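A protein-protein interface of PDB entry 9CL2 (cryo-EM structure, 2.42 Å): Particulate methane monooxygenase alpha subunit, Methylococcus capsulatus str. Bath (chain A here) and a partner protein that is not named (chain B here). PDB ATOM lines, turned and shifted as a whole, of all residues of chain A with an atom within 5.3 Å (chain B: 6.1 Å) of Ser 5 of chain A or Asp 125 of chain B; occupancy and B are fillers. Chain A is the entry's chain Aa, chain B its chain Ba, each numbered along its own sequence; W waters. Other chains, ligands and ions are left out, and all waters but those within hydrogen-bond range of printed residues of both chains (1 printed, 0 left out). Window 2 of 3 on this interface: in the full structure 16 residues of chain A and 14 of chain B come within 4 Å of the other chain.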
ATOM      1  N   GLY A   2     -10.951  12.394  30.051  1.00  0.00           N
ATOM      2  CA  GLY A   2     -11.970  13.315  29.490  1.00  0.00           C
ATOM      3  C   GLY A   2     -11.693  13.720  28.054  1.00  0.00           C
ATOM      4  O   GLY A   2     -12.571  14.378  27.468  1.00  0.00           O
ATOM      5  N   GLU A   3     -10.556  13.328  27.487  1.00  0.00           N
ATOM      6  CA  GLU A   3     -10.108  13.702  26.125  1.00  0.00           C
ATOM      7  C   GLU A   3     -10.678  12.691  25.122  1.00  0.00           C
ATOM      8  O   GLU A   3     -11.127  13.121  24.052  1.00  0.00           O
ATOM      9  CB  GLU A   3      -8.583  13.768  26.078  1.00  0.00           C
ATOM     10  CG  GLU A   3      -7.884  12.469  26.472  1.00  0.00           C
ATOM     11  CD  GLU A   3      -7.525  12.360  27.941  1.00  0.00           C
ATOM     12  OE1 GLU A   3      -8.023  13.181  28.737  1.00  0.00           O
ATOM     13  OE2 GLU A   3      -6.747  11.450  28.287  1.00  0.00           O
ATOM     14  N   LYS A   4     -10.685  11.408  25.470  1.00  0.00           N
ATOM     15  CA  LYS A   4     -11.140  10.374  24.509  1.00  0.00           C
ATOM     16  C   LYS A   4     -12.554  10.708  24.018  1.00  0.00           C
ATOM     17  O   LYS A   4     -12.866  10.369  22.865  1.00  0.00           O
ATOM     18  CB  LYS A   4     -11.059   9.001  25.179  1.00  0.00           C
ATOM     19  CG  LYS A   4      -9.672   8.392  25.219  1.00  0.00           C
ATOM     20  CD  LYS A   4      -9.641   7.127  26.063  1.00  0.00           C
ATOM     21  CE  LYS A   4      -8.470   7.117  26.984  1.00  0.00           C
ATOM     22  NZ  LYS A   4      -7.462   6.162  26.524  1.00  0.00           N
ATOM     23  N   SER A   5     -13.359  11.372  24.844  1.00  0.00           N
ATOM     24  CA  SER A   5     -14.768  11.667  24.482  1.00  0.00           C
ATOM     25  C   SER A   5     -14.877  12.989  23.713  1.00  0.00           C
ATOM     26  O   SER A   5     -15.974  13.276  23.204  1.00  0.00           O
ATOM     27  CB  SER A   5     -15.622  11.708  25.708  1.00  0.00           C
ATOM     28  OG  SER A   5     -14.936  11.161  26.825  1.00  0.00           O
ATOM     29  N   GLN A   6     -13.792  13.759  23.638  1.00  0.00           N
ATOM     30  CA  GLN A   6     -13.813  15.037  22.887  1.00  0.00           C
ATOM     31  C   GLN A   6     -13.678  14.734  21.389  1.00  0.00           C
ATOM     32  O   GLN A   6     -12.981  13.762  21.048  1.00  0.00           O
ATOM     33  CB  GLN A   6     -12.716  15.981  23.374  1.00  0.00           C
ATOM     34  CG  GLN A   6     -12.952  16.532  24.775  1.00  0.00           C
ATOM     35  CD  GLN A   6     -11.908  17.540  25.198  1.00  0.00           C
ATOM     36  OE1 GLN A   6     -12.222  18.647  25.645  1.00  0.00           O
ATOM     37  NE2 GLN A   6     -10.647  17.163  25.058  1.00  0.00           N
ATOM     38  N   ALA A   7     -14.315  15.543  20.540  1.00  0.00           N
ATOM     39  CA  ALA A   7     -14.258  15.341  19.071  1.00  0.00           C
ATOM     40  C   ALA A   7     -12.810  15.256  18.596  1.00  0.00           C
ATOM     41  O   ALA A   7     -11.974  16.067  19.033  1.00  0.00           O
ATOM     42  CB  ALA A   7     -14.984  16.451  18.367  1.00  0.00           C
ATOM     43  N   ARG A  11      -9.657  18.105  18.999  1.00  0.00           N
ATOM     44  CA  ARG A  11      -8.379  17.786  19.624  1.00  0.00           C
ATOM     45  C   ARG A  11      -7.214  17.992  18.664  1.00  0.00           C
ATOM     46  O   ARG A  11      -6.121  18.379  19.090  1.00  0.00           O
ATOM     47  CB  ARG A  11      -8.404  16.346  20.130  1.00  0.00           C
ATOM     48  CG  ARG A  11      -9.204  16.150  21.403  1.00  0.00           C
ATOM     49  CD  ARG A  11      -9.137  14.710  21.863  1.00  0.00           C
ATOM     50  NE  ARG A  11      -9.519  13.798  20.792  1.00  0.00           N
ATOM     51  CZ  ARG A  11      -9.718  12.497  20.949  1.00  0.00           C
ATOM     52  NH1 ARG A  11      -9.570  11.913  22.125  1.00  0.00           N
ATOM     53  NH2 ARG A  11     -10.077  11.765  19.899  1.00  0.00           N
ATOM     54  N   ARG A 343      -9.646   7.139  20.409  1.00  0.00           N
ATOM     55  CA  ARG A 343     -10.837   7.484  19.591  1.00  0.00           C
ATOM     56  C   ARG A 343     -10.524   8.578  18.561  1.00  0.00           C
ATOM     57  O   ARG A 343     -11.372   9.464  18.378  1.00  0.00           O
ATOM     58  CB  ARG A 343     -11.956   7.851  20.569  1.00  0.00           C
ATOM     59  CG  ARG A 343     -12.471   6.725  21.451  1.00  0.00           C
ATOM     60  CD  ARG A 343     -13.960   6.922  21.646  1.00  0.00           C
ATOM     61  NE  ARG A 343     -14.274   8.342  21.829  1.00  0.00           N
ATOM     62  CZ  ARG A 343     -15.180   9.019  21.137  1.00  0.00           C
ATOM     63  NH1 ARG A 343     -16.297   8.426  20.762  1.00  0.00           N
ATOM     64  NH2 ARG A 343     -14.964  10.284  20.824  1.00  0.00           N
ATOM     65  N   GLY B  36     -14.574   5.302  37.899  1.00  0.00           N
ATOM     66  CA  GLY B  36     -15.480   6.319  37.394  1.00  0.00           C
ATOM     67  C   GLY B  36     -14.829   7.444  36.620  1.00  0.00           C
ATOM     68  O   GLY B  36     -15.538   8.222  35.974  1.00  0.00           O
ATOM     69  N   LEU B  37     -13.499   7.556  36.668  1.00  0.00           N
ATOM     70  CA  LEU B  37     -12.838   8.694  36.034  1.00  0.00           C
ATOM     71  C   LEU B  37     -12.857   8.585  34.513  1.00  0.00           C
ATOM     72  O   LEU B  37     -13.152   9.567  33.821  1.00  0.00           O
ATOM     73  CB  LEU B  37     -11.404   8.821  36.546  1.00  0.00           C
ATOM     74  CG  LEU B  37     -11.253   9.444  37.935  1.00  0.00           C
ATOM     75  CD1 LEU B  37      -9.888   9.127  38.525  1.00  0.00           C
ATOM     76  CD2 LEU B  37     -11.481  10.946  37.874  1.00  0.00           C
ATOM     77  N   ASP B  38     -12.550   7.409  33.975  1.00  0.00           N
ATOM     78  CA  ASP B  38     -12.492   7.190  32.536  1.00  0.00           C
ATOM     79  C   ASP B  38     -13.736   6.431  32.100  1.00  0.00           C
ATOM     80  O   ASP B  38     -14.053   5.380  32.665  1.00  0.00           O
ATOM     81  CB  ASP B  38     -11.231   6.413  32.150  1.00  0.00           C
ATOM     82  CG  ASP B  38     -10.876   6.565  30.682  1.00  0.00           C
ATOM     83  OD1 ASP B  38     -11.779   6.860  29.872  1.00  0.00           O
ATOM     84  OD2 ASP B  38      -9.688   6.386  30.337  1.00  0.00           O
ATOM     85  N   SER B  39     -14.431   6.957  31.092  1.00  0.00           N
ATOM     86  CA  SER B  39     -15.705   6.392  30.667  1.00  0.00           C
ATOM     87  C   SER B  39     -15.572   5.364  29.552  1.00  0.00           C
ATOM     88  O   SER B  39     -16.500   4.573  29.347  1.00  0.00           O
ATOM     89  CB  SER B  39     -16.649   7.507  30.209  1.00  0.00           C
ATOM     90  OG  SER B  39     -16.668   7.612  28.797  1.00  0.00           O
ATOM     91  N   PHE B  40     -14.451   5.354  28.828  1.00  0.00           N
ATOM     92  CA  PHE B  40     -14.225   4.403  27.745  1.00  0.00           C
ATOM     93  C   PHE B  40     -13.367   3.219  28.173  1.00  0.00           C
ATOM     94  O   PHE B  40     -12.555   2.727  27.378  1.00  0.00           O
ATOM     95  CB  PHE B  40     -13.597   5.111  26.545  1.00  0.00           C
ATOM     96  CG  PHE B  40     -14.558   5.979  25.786  1.00  0.00           C
ATOM     97  CD1 PHE B  40     -15.480   5.416  24.921  1.00  0.00           C
ATOM     98  CD2 PHE B  40     -14.542   7.355  25.939  1.00  0.00           C
ATOM     99  CE1 PHE B  40     -16.369   6.210  24.221  1.00  0.00           C
ATOM    100  CE2 PHE B  40     -15.427   8.152  25.242  1.00  0.00           C
ATOM    101  CZ  PHE B  40     -16.343   7.578  24.383  1.00  0.00           C
ATOM    102  N   PHE B  44     -15.017   0.835  34.180  1.00  0.00           N
ATOM    103  CA  PHE B  44     -16.124   1.784  34.205  1.00  0.00           C
ATOM    104  C   PHE B  44     -17.413   1.121  33.752  1.00  0.00           C
ATOM    105  O   PHE B  44     -18.466   1.297  34.374  1.00  0.00           O
ATOM    106  CB  PHE B  44     -15.814   2.988  33.320  1.00  0.00           C
ATOM    107  CG  PHE B  44     -16.916   4.011  33.285  1.00  0.00           C
ATOM    108  CD1 PHE B  44     -17.035   4.957  34.289  1.00  0.00           C
ATOM    109  CD2 PHE B  44     -17.837   4.022  32.250  1.00  0.00           C
ATOM    110  CE1 PHE B  44     -18.048   5.895  34.259  1.00  0.00           C
ATOM    111  CE2 PHE B  44     -18.851   4.958  32.215  1.00  0.00           C
ATOM    112  CZ  PHE B  44     -18.957   5.896  33.221  1.00  0.00           C
ATOM    113  N   ILE B 122     -13.544  17.405  38.248  1.00  0.00           N
ATOM    114  CA  ILE B 122     -13.037  16.640  37.115  1.00  0.00           C
ATOM    115  C   ILE B 122     -13.552  17.253  35.815  1.00  0.00           C
ATOM    116  O   ILE B 122     -14.389  18.155  35.814  1.00  0.00           O
ATOM    117  CB  ILE B 122     -13.403  15.140  37.199  1.00  0.00           C
ATOM    118  CG1 ILE B 122     -14.908  14.939  37.385  1.00  0.00           C
ATOM    119  CG2 ILE B 122     -12.633  14.465  38.325  1.00  0.00           C
ATOM    120  CD1 ILE B 122     -15.678  14.709  36.099  1.00  0.00           C
ATOM    121  N   VAL B 123     -13.032  16.744  34.702  1.00  0.00           N
ATOM    122  CA  VAL B 123     -13.474  17.140  33.369  1.00  0.00           C
ATOM    123  C   VAL B 123     -14.607  16.216  32.947  1.00  0.00           C
ATOM    124  O   VAL B 123     -14.461  14.989  32.972  1.00  0.00           O
ATOM    125  CB  VAL B 123     -12.318  17.088  32.358  1.00  0.00           C
ATOM    126  CG1 VAL B 123     -12.853  17.181  30.937  1.00  0.00           C
ATOM    127  CG2 VAL B 123     -11.331  18.205  32.620  1.00  0.00           C
ATOM    128  N   ARG B 124     -15.737  16.804  32.565  1.00  0.00           N
ATOM    129  CA  ARG B 124     -16.886  16.017  32.140  1.00  0.00           C
ATOM    130  C   ARG B 124     -16.575  15.291  30.837  1.00  0.00           C
ATOM    131  O   ARG B 124     -16.017  15.877  29.904  1.00  0.00           O
ATOM    132  CB  ARG B 124     -18.103  16.922  31.970  1.00  0.00           C
ATOM    133  CG  ARG B 124     -19.423  16.258  32.302  1.00  0.00           C
ATOM    134  CD  ARG B 124     -20.375  17.260  32.925  1.00  0.00           C
ATOM    135  NE  ARG B 124     -21.754  17.045  32.507  1.00  0.00           N
ATOM    136  CZ  ARG B 124     -22.793  17.709  32.996  1.00  0.00           C
ATOM    137  NH1 ARG B 124     -22.644  18.634  33.929  1.00  0.00           N
ATOM    138  NH2 ARG B 124     -24.010  17.439  32.534  1.00  0.00           N
ATOM    139  N   ASP B 125     -16.936  14.010  30.775  1.00  0.00           N
ATOM    140  CA  ASP B 125     -16.662  13.177  29.611  1.00  0.00           C
ATOM    141  C   ASP B 125     -17.918  12.593  28.984  1.00  0.00           C
ATOM    142  O   ASP B 125     -18.003  12.484  27.759  1.00  0.00           O
ATOM    143  CB  ASP B 125     -15.698  12.042  29.992  1.00  0.00           C
ATOM    144  CG  ASP B 125     -15.981  11.476  31.368  1.00  0.00           C
ATOM    145  OD1 ASP B 125     -17.013  11.847  31.966  1.00  0.00           O
ATOM    146  OD2 ASP B 125     -15.171  10.657  31.853  1.00  0.00           O
ATOM    147  N   THR B 126     -18.904  12.206  29.790  1.00  0.00           N
ATOM    148  CA  THR B 126     -20.115  11.590  29.270  1.00  0.00           C
ATOM    149  C   THR B 126     -21.315  12.109  30.048  1.00  0.00           C
ATOM    150  O   THR B 126     -21.177  12.768  31.084  1.00  0.00           O
ATOM    151  CB  THR B 126     -20.042  10.061  29.351  1.00  0.00           C
ATOM    152  OG1 THR B 126     -21.348   9.508  29.157  1.00  0.00           O
ATOM    153  CG2 THR B 126     -19.518   9.630  30.709  1.00  0.00           C
ATOM    154  N   ASP B 127     -22.508  11.810  29.534  1.00  0.00           N
ATOM    155  CA  ASP B 127     -23.727  12.107  30.272  1.00  0.00           C
ATOM    156  C   ASP B 127     -23.963  11.102  31.391  1.00  0.00           C
ATOM    157  O   ASP B 127     -24.675  11.407  32.353  1.00  0.00           O
ATOM    158  CB  ASP B 127     -24.928  12.126  29.326  1.00  0.00           C
ATOM    159  CG  ASP B 127     -24.714  13.031  28.129  1.00  0.00           C
ATOM    160  OD1 ASP B 127     -23.994  14.042  28.265  1.00  0.00           O
ATOM    161  OD2 ASP B 127     -25.268  12.731  27.051  1.00  0.00           O
ATOM    162  N   THR B 129     -22.055   9.928  33.904  1.00  0.00           N
ATOM    163  CA  THR B 129     -21.047   9.921  34.947  1.00  0.00           C
ATOM    164  C   THR B 129     -21.594   9.190  36.169  1.00  0.00           C
ATOM    165  O   THR B 129     -22.811   9.095  36.349  1.00  0.00           O
ATOM    166  CB  THR B 129     -20.640  11.346  35.318  1.00  0.00           C
ATOM    167  OG1 THR B 129     -21.753  12.029  35.910  1.00  0.00           O
ATOM    168  CG2 THR B 129     -20.175  12.109  34.090  1.00  0.00           C
HETATM  169  O   HOH W   1     -10.644   9.776  29.213  1.00  0.00           O
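The backbone carbonyl oxygen of Asp 125 of chain B sits close to the side-chain hydroxyl of Ser 5 of chain A (3.5 Å).
Of the 8 printed residues of chain A, 4 touch a printed residue of chain B.
Along chain A the printed residues that touch a printed residue of chain B span positions 2 to 343.
Of the 13 printed residues of chain B, 3 touch a printed residue of chain A.
Hydrophobic or aromatic side chains of chain B within 4 Å of the printed part of chain A: Phe 40.
Among the printed residues, 6 pairs touch across the chains.
Among the printed residues, no Asp or Glu carboxylate lies within 4 Å of a Lys or Arg side-chain nitrogen of the other chain.
Of the printed residues of chain B, Gly 2 of chain A touches Asp 125.
Of the printed residues of chain B, Lys 4 of chain A touches Asp 38 and Phe 40.
Ser 5 of chain A touches just these residues of chain B: Phe 40 (3.4 Å) and Asp 125 (3.2 Å).
Gly 36 of chain B touches none of the printed residues of chain A.
Printed residues of chain A within 4 Å of Asp 38 of chain B: Lys 4 (3.6 Å).
Of chain A, only Gly 2 and Ser 5 come within 4 Å of Asp 125 of chain B.
The nearest printed residue of chain A that does not touch Asp 125 of chain B is Glu 3 of chain A (5.9 Å).
The nearest printed residue of chain B that does not touch Gly 2 of chain A is Val 123 of chain B (4.2 Å).
Among the printed residues, pairs that only touch across the chains: Arg 343 of chain A with Phe 40 of chain B (3.4 Å), Ser 5 of chain A with Phe 40 of chain B (3.4 Å), Lys 4 of chain A with Asp 38 of chain B (3.6 Å), Lys 4 of chain A with Phe 40 of chain B (3.9 Å) and Gly 2 of chain A with Asp 125 of chain B (3.97 Å).
Water W1 bridges the backbone NH (N) of Gly 2 of chain A (2.8 Å) and the side-chain carboxylate (OD1) of Asp 38 of chain B (3.2 Å).
The backbone NH (N) of Phe 40 of chain B lies within hydrogen-bond range of the side-chain carboxylate (OD1) of Asp 38 of chain B, at 3.2 Å.
O of Lys 4 of chain A sits at hydrogen-bond distance from NE of Arg 343 of chain A, 2.7 Å away.
NH2 of Arg 11 of chain A is in hydrogen-bond range of O of Arg 343 of chain A, 3.0 Å away.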
